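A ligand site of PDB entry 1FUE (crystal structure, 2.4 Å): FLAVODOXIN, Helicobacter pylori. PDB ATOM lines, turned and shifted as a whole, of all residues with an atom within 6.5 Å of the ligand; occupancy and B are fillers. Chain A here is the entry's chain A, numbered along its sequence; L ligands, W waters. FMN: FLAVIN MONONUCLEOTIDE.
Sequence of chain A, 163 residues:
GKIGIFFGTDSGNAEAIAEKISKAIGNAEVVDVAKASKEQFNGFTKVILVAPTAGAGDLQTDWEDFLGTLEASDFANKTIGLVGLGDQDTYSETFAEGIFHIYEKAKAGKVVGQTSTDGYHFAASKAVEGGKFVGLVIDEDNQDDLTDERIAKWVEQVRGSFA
Water W1 lies within hydrogen-bond range of N of Glu 140 (2.6 Å), OD2 of Asp 141 (2.6 Å), O4' of the ligand (2.9 Å) and O of Gly 86 (3.1 Å).
The side-chain hydroxyl (OG1) of Thr 9 sits at hydrogen-bond distance from the backbone NH (N) of Gly 12 (2.8 Å). N of Asp 141 sits close to OD1 of Asp 139, 3.5 Å away. The side-chain hydroxyl (OG1) of Thr 53 is in hydrogen-bond range of the backbone carbonyl oxygen (O) of Leu 85 (2.8 Å). The backbone NH (N) of Glu 97 lies within hydrogen-bond range of the side-chain hydroxyl (OG1) of Thr 53 (3.3 Å). The side-chain amide nitrogen (NE2) of Gln 60 sits at hydrogen-bond distance from the side-chain carboxylate (OD1) of Asp 10 (3.1 Å). The backbone NH (N) of Gly 86 sits at hydrogen-bond distance from the backbone carbonyl oxygen (O) of Ile 138 (2.9 Å).
The side-chain hydroxyl (OG1) of Thr 9 is in hydrogen-bond range of an oxygen (O3P) of the ligand, 2.4 Å away. The side-chain carboxylate (OD2) of Asp 141 lies within hydrogen-bond range of an oxygen (O3') of the ligand, 2.4 Å away. The backbone NH of Ser 11 sits at hydrogen-bond distance from an oxygen (O2P) of the ligand (3.1 Å). O1P of the ligand sits close to OG of Ser 11 (3.2 Å). N of Ala 14 sits at hydrogen-bond distance from O3P of the ligand. The backbone carbonyl oxygen (O) of Thr 94 lies within hydrogen-bond range of a nitrogen (N3) of the ligand (3.0 Å). The backbone NH (N) of Asp 87 sits at hydrogen-bond distance from an oxygen (O2) of the ligand, 3.0 Å away. The backbone NH (N) of Thr 53 lies within hydrogen-bond range of an oxygen (O2') of the ligand (3.5 Å). O2' of the ligand lies within hydrogen-bond range of O of Thr 53, at 3.0 Å. O2P of the ligand sits at hydrogen-bond distance from N of Asp 10 (3.0 Å). An oxygen (O2) of the ligand is in hydrogen-bond range of the backbone NH of Ala 96. The backbone NH (N) of Asn 13 is in hydrogen-bond range of an oxygen (O1P) of the ligand (3.2 Å). OD1 of Asn 13 sits at hydrogen-bond distance from O4' of the ligand (3.1 Å). O4 of the ligand sits at hydrogen-bond distance from N of Gly 57. N of Gly 55 lies close to N5 of the ligand. The backbone NH of Gly 12 is in hydrogen-bond range of an oxygen (O1P) of the ligand (3.3 Å). The backbone carbonyl oxygen (O) of Leu 85 sits at hydrogen-bond distance from an oxygen (O2') of the ligand, at 3.4 Å.
The backbone carbonyl oxygen of Ala 54 lies close to an oxygen (O4) of the ligand, 3.0 Å away. Pro 52 touches the ligand (CB to O5', 3.3 Å). Ala 56 touches the ligand. Gly 86 touches the ligand (CA to O2, 3.3 Å). Tyr 91 touches the ligand. Phe 95 touches the ligand (CA to O2, 3.5 Å). Hydrophobic or aromatic side chains that line the ligand: Ala 14, Pro 52, Leu 85, Tyr 91 and Phe 95. Within 4 Å of the ligand: Thr 9, Asp 10, Ser 11, Gly 12, Asn 13, Ala 14, Pro 52, Thr 53, Ala 54, Gly 55, Ala 56, Gly 57, Leu 85, Gly 86, Asp 87, Tyr 91, Thr 94, Phe 95, Ala 96 and Asp 141. The nearest printed residue that does not touch the ligand is Gly 8 (4.5 Å).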
ATOM      1  N   GLY A   8     -14.821  19.820  -5.613  1.00  0.00           N
ATOM      2  CA  GLY A   8     -15.286  18.882  -6.609  1.00  0.00           C
ATOM      3  C   GLY A   8     -14.784  17.538  -6.141  1.00  0.00           C
ATOM      4  O   GLY A   8     -13.639  17.437  -5.720  1.00  0.00           O
ATOM      5  N   THR A   9     -15.612  16.499  -6.203  1.00  0.00           N
ATOM      6  CA  THR A   9     -15.153  15.192  -5.736  1.00  0.00           C
ATOM      7  C   THR A   9     -15.761  13.992  -6.434  1.00  0.00           C
ATOM      8  O   THR A   9     -16.831  14.072  -7.038  1.00  0.00           O
ATOM      9  CB  THR A   9     -15.430  15.018  -4.224  1.00  0.00           C
ATOM     10  OG1 THR A   9     -14.862  13.793  -3.767  1.00  0.00           O
ATOM     11  CG2 THR A   9     -16.933  14.990  -3.955  1.00  0.00           C
ATOM     12  N   ASP A  10     -15.069  12.865  -6.333  1.00  0.00           N
ATOM     13  CA  ASP A  10     -15.540  11.614  -6.884  1.00  0.00           C
ATOM     14  C   ASP A  10     -15.827  10.644  -5.748  1.00  0.00           C
ATOM     15  O   ASP A  10     -16.920  10.092  -5.677  1.00  0.00           O
ATOM     16  CB  ASP A  10     -14.509  11.010  -7.846  1.00  0.00           C
ATOM     17  CG  ASP A  10     -14.466  11.750  -9.173  1.00  0.00           C
ATOM     18  OD1 ASP A  10     -15.521  12.237  -9.620  1.00  0.00           O
ATOM     19  OD2 ASP A  10     -13.375  11.813  -9.774  1.00  0.00           O
ATOM     20  N   SER A  11     -14.854  10.442  -4.861  1.00  0.00           N
ATOM     21  CA  SER A  11     -15.035   9.532  -3.727  1.00  0.00           C
ATOM     22  C   SER A  11     -15.707  10.241  -2.563  1.00  0.00           C
ATOM     23  O   SER A  11     -16.643   9.719  -1.954  1.00  0.00           O
ATOM     24  CB  SER A  11     -13.695   8.971  -3.245  1.00  0.00           C
ATOM     25  OG  SER A  11     -12.928   8.460  -4.304  1.00  0.00           O
ATOM     26  N   GLY A  12     -15.235  11.442  -2.250  1.00  0.00           N
ATOM     27  CA  GLY A  12     -15.829  12.181  -1.167  1.00  0.00           C
ATOM     28  C   GLY A  12     -14.805  12.868  -0.295  1.00  0.00           C
ATOM     29  O   GLY A  12     -15.147  13.704   0.533  1.00  0.00           O
ATOM     30  N   ASN A  13     -13.539  12.525  -0.495  1.00  0.00           N
ATOM     31  CA  ASN A  13     -12.470  13.137   0.291  1.00  0.00           C
ATOM     32  C   ASN A  13     -12.512  14.659   0.220  1.00  0.00           C
ATOM     33  O   ASN A  13     -12.547  15.333   1.251  1.00  0.00           O
ATOM     34  CB  ASN A  13     -11.106  12.641  -0.186  1.00  0.00           C
ATOM     35  CG  ASN A  13     -10.866  11.176   0.131  1.00  0.00           C
ATOM     36  OD1 ASN A  13     -10.066  10.512  -0.526  1.00  0.00           O
ATOM     37  ND2 ASN A  13     -11.565  10.664   1.147  1.00  0.00           N
ATOM     38  N   ALA A  14     -12.533  15.199  -0.995  1.00  0.00           N
ATOM     39  CA  ALA A  14     -12.555  16.647  -1.148  1.00  0.00           C
ATOM     40  C   ALA A  14     -13.717  17.278  -0.385  1.00  0.00           C
ATOM     41  O   ALA A  14     -13.530  18.253   0.325  1.00  0.00           O
ATOM     42  CB  ALA A  14     -12.644  17.033  -2.624  1.00  0.00           C
ATOM     43  N   GLU A  15     -14.909  16.702  -0.534  1.00  0.00           N
ATOM     44  CA  GLU A  15     -16.086  17.233   0.146  1.00  0.00           C
ATOM     45  C   GLU A  15     -15.846  17.279   1.634  1.00  0.00           C
ATOM     46  O   GLU A  15     -16.169  18.266   2.304  1.00  0.00           O
ATOM     47  CB  GLU A  15     -17.300  16.342  -0.144  1.00  0.00           C
ATOM     48  CG  GLU A  15     -18.589  16.834   0.510  1.00  0.00           C
ATOM     49  CD  GLU A  15     -19.806  16.025   0.103  1.00  0.00           C
ATOM     50  OE1 GLU A  15     -20.011  15.829  -1.118  1.00  0.00           O
ATOM     51  OE2 GLU A  15     -20.560  15.583   0.990  1.00  0.00           O
ATOM     52  N   PRO A  52      -9.330  17.713  -6.033  1.00  0.00           N
ATOM     53  CA  PRO A  52      -8.574  16.467  -6.037  1.00  0.00           C
ATOM     54  C   PRO A  52      -7.903  16.311  -7.412  1.00  0.00           C
ATOM     55  O   PRO A  52      -8.388  16.839  -8.416  1.00  0.00           O
ATOM     56  CB  PRO A  52      -9.643  15.417  -5.777  1.00  0.00           C
ATOM     57  CG  PRO A  52     -10.852  16.003  -6.439  1.00  0.00           C
ATOM     58  CD  PRO A  52     -10.784  17.449  -6.016  1.00  0.00           C
ATOM     59  N   THR A  53      -6.781  15.596  -7.463  1.00  0.00           N
ATOM     60  CA  THR A  53      -6.045  15.413  -8.706  1.00  0.00           C
ATOM     61  C   THR A  53      -6.443  14.140  -9.458  1.00  0.00           C
ATOM     62  O   THR A  53      -6.358  13.040  -8.919  1.00  0.00           O
ATOM     63  CB  THR A  53      -4.556  15.336  -8.440  1.00  0.00           C
ATOM     64  OG1 THR A  53      -4.171  16.428  -7.607  1.00  0.00           O
ATOM     65  CG2 THR A  53      -3.793  15.392  -9.745  1.00  0.00           C
ATOM     66  N   ALA A  54      -6.884  14.305 -10.709  1.00  0.00           N
ATOM     67  CA  ALA A  54      -7.286  13.171 -11.534  1.00  0.00           C
ATOM     68  C   ALA A  54      -6.073  12.540 -12.222  1.00  0.00           C
ATOM     69  O   ALA A  54      -4.940  13.012 -12.075  1.00  0.00           O
ATOM     70  CB  ALA A  54      -8.315  13.619 -12.583  1.00  0.00           C
ATOM     71  N   GLY A  55      -6.319  11.481 -12.975  1.00  0.00           N
ATOM     72  CA  GLY A  55      -5.241  10.798 -13.668  1.00  0.00           C
ATOM     73  C   GLY A  55      -4.407  11.720 -14.535  1.00  0.00           C
ATOM     74  O   GLY A  55      -4.939  12.635 -15.158  1.00  0.00           O
ATOM     75  N   ALA A  56      -3.103  11.472 -14.568  1.00  0.00           N
ATOM     76  CA  ALA A  56      -2.184  12.264 -15.368  1.00  0.00           C
ATOM     77  C   ALA A  56      -1.872  13.622 -14.746  1.00  0.00           C
ATOM     78  O   ALA A  56      -1.001  14.362 -15.224  1.00  0.00           O
ATOM     79  CB  ALA A  56      -2.746  12.451 -16.773  1.00  0.00           C
ATOM     80  N   GLY A  57      -2.575  13.955 -13.669  1.00  0.00           N
ATOM     81  CA  GLY A  57      -2.337  15.231 -13.019  1.00  0.00           C
ATOM     82  C   GLY A  57      -3.394  16.244 -13.396  1.00  0.00           C
ATOM     83  O   GLY A  57      -3.307  17.420 -12.998  1.00  0.00           O
ATOM     84  N   ASP A  58      -4.388  15.793 -14.143  1.00  0.00           N
ATOM     85  CA  ASP A  58      -5.456  16.678 -14.569  1.00  0.00           C
ATOM     86  C   ASP A  58      -6.533  16.847 -13.497  1.00  0.00           C
ATOM     87  O   ASP A  58      -6.592  16.091 -12.523  1.00  0.00           O
ATOM     88  CB  ASP A  58      -6.063  16.182 -15.877  1.00  0.00           C
ATOM     89  CG  ASP A  58      -5.038  16.127 -16.996  1.00  0.00           C
ATOM     90  OD1 ASP A  58      -4.211  17.070 -17.083  1.00  0.00           O
ATOM     91  OD2 ASP A  58      -5.049  15.164 -17.782  1.00  0.00           O
ATOM     92  N   GLN A  60     -10.153  16.994 -11.565  1.00  0.00           N
ATOM     93  CA  GLN A  60     -11.300  16.130 -11.340  1.00  0.00           C
ATOM     94  C   GLN A  60     -12.326  16.643 -12.350  1.00  0.00           C
ATOM     95  O   GLN A  60     -12.372  17.840 -12.640  1.00  0.00           O
ATOM     96  CB  GLN A  60     -11.768  16.329  -9.899  1.00  0.00           C
ATOM     97  CG  GLN A  60     -12.934  15.481  -9.404  1.00  0.00           C
ATOM     98  CD  GLN A  60     -14.280  16.117  -9.700  1.00  0.00           C
ATOM     99  OE1 GLN A  60     -14.440  17.342  -9.668  1.00  0.00           O
ATOM    100  NE2 GLN A  60     -15.261  15.275  -9.980  1.00  0.00           N
ATOM    101  N   LEU A  85      -5.713  17.806  -3.459  1.00  0.00           N
ATOM    102  CA  LEU A  85      -5.650  16.467  -2.889  1.00  0.00           C
ATOM    103  C   LEU A  85      -4.812  15.582  -3.820  1.00  0.00           C
ATOM    104  O   LEU A  85      -4.917  15.686  -5.043  1.00  0.00           O
ATOM    105  CB  LEU A  85      -7.043  15.872  -2.767  1.00  0.00           C
ATOM    106  CG  LEU A  85      -7.987  16.306  -1.655  1.00  0.00           C
ATOM    107  CD1 LEU A  85      -9.368  15.762  -1.937  1.00  0.00           C
ATOM    108  CD2 LEU A  85      -7.482  15.779  -0.327  1.00  0.00           C
ATOM    109  N   GLY A  86      -4.008  14.704  -3.238  1.00  0.00           N
ATOM    110  CA  GLY A  86      -3.189  13.822  -4.068  1.00  0.00           C
ATOM    111  C   GLY A  86      -2.689  12.556  -3.381  1.00  0.00           C
ATOM    112  O   GLY A  86      -2.817  12.389  -2.167  1.00  0.00           O
ATOM    113  N   ASP A  87      -2.089  11.683  -4.182  1.00  0.00           N
ATOM    114  CA  ASP A  87      -1.545  10.416  -3.704  1.00  0.00           C
ATOM    115  C   ASP A  87      -0.049  10.435  -4.065  1.00  0.00           C
ATOM    116  O   ASP A  87       0.326  10.001  -5.151  1.00  0.00           O
ATOM    117  CB  ASP A  87      -2.227   9.260  -4.428  1.00  0.00           C
ATOM    118  CG  ASP A  87      -1.954   7.909  -3.786  1.00  0.00           C
ATOM    119  OD1 ASP A  87      -0.947   7.772  -3.044  1.00  0.00           O
ATOM    120  OD2 ASP A  87      -2.742   6.982  -4.047  1.00  0.00           O
ATOM    121  N   GLN A  88       0.764  10.940  -3.144  1.00  0.00           N
ATOM    122  CA  GLN A  88       2.204  11.057  -3.354  1.00  0.00           C
ATOM    123  C   GLN A  88       2.978   9.749  -3.522  1.00  0.00           C
ATOM    124  O   GLN A  88       4.040   9.742  -4.135  1.00  0.00           O
ATOM    125  CB  GLN A  88       2.839  11.851  -2.214  1.00  0.00           C
ATOM    126  CG  GLN A  88       2.653  11.224  -0.848  1.00  0.00           C
ATOM    127  CD  GLN A  88       3.051  12.154   0.273  1.00  0.00           C
ATOM    128  OE1 GLN A  88       4.234  12.302   0.589  1.00  0.00           O
ATOM    129  NE2 GLN A  88       2.073  12.809   0.883  1.00  0.00           N
ATOM    130  N   TYR A  91       1.456   8.185  -7.052  1.00  0.00           N
ATOM    131  CA  TYR A  91       1.713   9.115  -8.154  1.00  0.00           C
ATOM    132  C   TYR A  91       2.822  10.095  -7.813  1.00  0.00           C
ATOM    133  O   TYR A  91       2.589  11.302  -7.729  1.00  0.00           O
ATOM    134  CB  TYR A  91       0.439   9.896  -8.476  1.00  0.00           C
ATOM    135  CG  TYR A  91      -0.758   9.014  -8.733  1.00  0.00           C
ATOM    136  CD1 TYR A  91      -1.062   8.579 -10.011  1.00  0.00           C
ATOM    137  CD2 TYR A  91      -1.576   8.599  -7.681  1.00  0.00           C
ATOM    138  CE1 TYR A  91      -2.163   7.763 -10.253  1.00  0.00           C
ATOM    139  CE2 TYR A  91      -2.679   7.778  -7.899  1.00  0.00           C
ATOM    140  CZ  TYR A  91      -2.972   7.363  -9.197  1.00  0.00           C
ATOM    141  OH  TYR A  91      -4.074   6.562  -9.439  1.00  0.00           O
ATOM    142  N   THR A  94       3.335  13.492 -10.187  1.00  0.00           N
ATOM    143  CA  THR A  94       2.080  14.130 -10.571  1.00  0.00           C
ATOM    144  C   THR A  94       1.364  14.455  -9.276  1.00  0.00           C
ATOM    145  O   THR A  94       0.143  14.621  -9.252  1.00  0.00           O
ATOM    146  CB  THR A  94       1.203  13.149 -11.391  1.00  0.00           C
ATOM    147  OG1 THR A  94       1.820  12.885 -12.646  1.00  0.00           O
ATOM    148  CG2 THR A  94      -0.141  13.729 -11.652  1.00  0.00           C
ATOM    149  N   PHE A  95       2.116  14.556  -8.193  1.00  0.00           N
ATOM    150  CA  PHE A  95       1.521  14.820  -6.895  1.00  0.00           C
ATOM    151  C   PHE A  95       0.694  16.101  -6.754  1.00  0.00           C
ATOM    152  O   PHE A  95       1.238  17.206  -6.751  1.00  0.00           O
ATOM    153  CB  PHE A  95       2.582  14.797  -5.801  1.00  0.00           C
ATOM    154  CG  PHE A  95       2.027  14.949  -4.412  1.00  0.00           C
ATOM    155  CD1 PHE A  95       0.932  14.187  -4.004  1.00  0.00           C
ATOM    156  CD2 PHE A  95       2.578  15.852  -3.514  1.00  0.00           C
ATOM    157  CE1 PHE A  95       0.412  14.320  -2.724  1.00  0.00           C
ATOM    158  CE2 PHE A  95       2.058  16.000  -2.234  1.00  0.00           C
ATOM    159  CZ  PHE A  95       0.981  15.230  -1.840  1.00  0.00           C
ATOM    160  N   ALA A  96      -0.614  15.919  -6.647  1.00  0.00           N
ATOM    161  CA  ALA A  96      -1.552  17.021  -6.477  1.00  0.00           C
ATOM    162  C   ALA A  96      -1.361  18.147  -7.471  1.00  0.00           C
ATOM    163  O   ALA A  96      -1.162  19.304  -7.092  1.00  0.00           O
ATOM    164  CB  ALA A  96      -1.421  17.558  -5.062  1.00  0.00           C
ATOM    165  N   GLU A  97      -1.418  17.822  -8.760  1.00  0.00           N
ATOM    166  CA  GLU A  97      -1.220  18.834  -9.793  1.00  0.00           C
ATOM    167  C   GLU A  97      -2.490  19.570 -10.206  1.00  0.00           C
ATOM    168  O   GLU A  97      -2.408  20.648 -10.783  1.00  0.00           O
ATOM    169  CB  GLU A  97      -0.586  18.223 -11.030  1.00  0.00           C
ATOM    170  CG  GLU A  97       0.743  17.557 -10.789  1.00  0.00           C
ATOM    171  CD  GLU A  97       1.614  17.596 -12.019  1.00  0.00           C
ATOM    172  OE1 GLU A  97       1.055  17.473 -13.144  1.00  0.00           O
ATOM    173  OE2 GLU A  97       2.844  17.753 -11.854  1.00  0.00           O
ATOM    174  N   ILE A 138      -3.139  18.040   0.485  1.00  0.00           N
ATOM    175  CA  ILE A 138      -3.592  17.006   1.400  1.00  0.00           C
ATOM    176  C   ILE A 138      -3.483  15.619   0.795  1.00  0.00           C
ATOM    177  O   ILE A 138      -3.697  15.431  -0.407  1.00  0.00           O
ATOM    178  CB  ILE A 138      -5.069  17.243   1.822  1.00  0.00           C
ATOM    179  CG1 ILE A 138      -5.175  18.530   2.650  1.00  0.00           C
ATOM    180  CG2 ILE A 138      -5.589  16.060   2.620  1.00  0.00           C
ATOM    181  CD1 ILE A 138      -4.554  18.454   4.033  1.00  0.00           C
ATOM    182  N   ASP A 139      -3.160  14.654   1.638  1.00  0.00           N
ATOM    183  CA  ASP A 139      -3.020  13.270   1.210  1.00  0.00           C
ATOM    184  C   ASP A 139      -3.912  12.459   2.129  1.00  0.00           C
ATOM    185  O   ASP A 139      -3.589  12.281   3.303  1.00  0.00           O
ATOM    186  CB  ASP A 139      -1.567  12.810   1.378  1.00  0.00           C
ATOM    187  CG  ASP A 139      -1.214  11.660   0.475  1.00  0.00           C
ATOM    188  OD1 ASP A 139      -2.111  10.876   0.084  1.00  0.00           O
ATOM    189  OD2 ASP A 139      -0.013  11.528   0.149  1.00  0.00           O
ATOM    190  N   GLU A 140      -5.043  11.977   1.615  1.00  0.00           N
ATOM    191  CA  GLU A 140      -5.957  11.191   2.426  1.00  0.00           C
ATOM    192  C   GLU A 140      -5.763   9.692   2.232  1.00  0.00           C
ATOM    193  O   GLU A 140      -6.311   8.884   2.973  1.00  0.00           O
ATOM    194  CB  GLU A 140      -7.409  11.570   2.125  1.00  0.00           C
ATOM    195  CG  GLU A 140      -7.811  12.945   2.663  1.00  0.00           C
ATOM    196  CD  GLU A 140      -7.270  13.190   4.061  1.00  0.00           C
ATOM    197  OE1 GLU A 140      -6.067  13.482   4.197  1.00  0.00           O
ATOM    198  OE2 GLU A 140      -8.043  13.084   5.041  1.00  0.00           O
ATOM    199  N   ASP A 141      -4.983   9.337   1.221  1.00  0.00           N
ATOM    200  CA  ASP A 141      -4.712   7.932   0.951  1.00  0.00           C
ATOM    201  C   ASP A 141      -3.420   7.522   1.657  1.00  0.00           C
ATOM    202  O   ASP A 141      -3.188   6.337   1.893  1.00  0.00           O
ATOM    203  CB  ASP A 141      -4.541   7.714  -0.551  1.00  0.00           C
ATOM    204  CG  ASP A 141      -5.709   8.245  -1.357  1.00  0.00           C
ATOM    205  OD1 ASP A 141      -6.766   7.574  -1.421  1.00  0.00           O
ATOM    206  OD2 ASP A 141      -5.570   9.356  -1.913  1.00  0.00           O
HETATM  207  N1  FMN L   1      -3.302  11.632  -7.100  1.00  0.00           N
HETATM  208  C2  FMN L   1      -2.224  12.380  -7.517  1.00  0.00           C
HETATM  209  O2  FMN L   1      -1.505  12.983  -6.779  1.00  0.00           O
HETATM  210  N3  FMN L   1      -1.936  12.450  -8.930  1.00  0.00           N
HETATM  211  C4  FMN L   1      -2.653  11.826  -9.906  1.00  0.00           C
HETATM  212  O4  FMN L   1      -2.340  11.937 -11.108  1.00  0.00           O
HETATM  213  C4A FMN L   1      -3.798  11.032  -9.450  1.00  0.00           C
HETATM  214  N5  FMN L   1      -4.545  10.399 -10.330  1.00  0.00           N
HETATM  215  C5A FMN L   1      -5.613   9.665  -9.908  1.00  0.00           C
HETATM  216  C6  FMN L   1      -6.442   8.960 -10.892  1.00  0.00           C
HETATM  217  C7  FMN L   1      -7.527   8.203 -10.567  1.00  0.00           C
HETATM  218  C7M FMN L   1      -8.387   7.476 -11.622  1.00  0.00           C
HETATM  219  C8  FMN L   1      -7.898   8.066  -9.130  1.00  0.00           C
HETATM  220  C8M FMN L   1      -9.087   7.237  -8.720  1.00  0.00           C
HETATM  221  C9  FMN L   1      -7.117   8.729  -8.186  1.00  0.00           C
HETATM  222  C9A FMN L   1      -5.988   9.527  -8.506  1.00  0.00           C
HETATM  223  N10 FMN L   1      -5.157  10.230  -7.569  1.00  0.00           N
HETATM  224  C10 FMN L   1      -4.067  10.984  -7.988  1.00  0.00           C
HETATM  225  C1' FMN L   1      -5.447  10.176  -6.110  1.00  0.00           C
HETATM  226  C2' FMN L   1      -6.418  11.278  -5.709  1.00  0.00           C
HETATM  227  O2' FMN L   1      -5.925  12.582  -6.006  1.00  0.00           O
HETATM  228  C3' FMN L   1      -6.746  11.262  -4.200  1.00  0.00           C
HETATM  229  O3' FMN L   1      -7.049   9.890  -3.774  1.00  0.00           O
HETATM  230  C4' FMN L   1      -7.910  12.158  -3.827  1.00  0.00           C
HETATM  231  O4' FMN L   1      -8.109  12.092  -2.391  1.00  0.00           O
HETATM  232  C5' FMN L   1      -9.251  11.779  -4.473  1.00  0.00           C
HETATM  233  O5' FMN L   1     -10.263  12.707  -4.045  1.00  0.00           O
HETATM  234  P   FMN L   1     -11.816  12.391  -4.014  1.00  0.00           P
HETATM  235  O1P FMN L   1     -12.022  11.250  -3.058  1.00  0.00           O
HETATM  236  O2P FMN L   1     -12.271  12.113  -5.428  1.00  0.00           O
HETATM  237  O3P FMN L   1     -12.459  13.732  -3.474  1.00  0.00           O
HETATM  238  O   HOH W   1      -5.638  11.814  -0.937  1.00  0.00           O
HETATM  239  O   HOH W   2      -9.097   8.147  -5.299  1.00  0.00           O
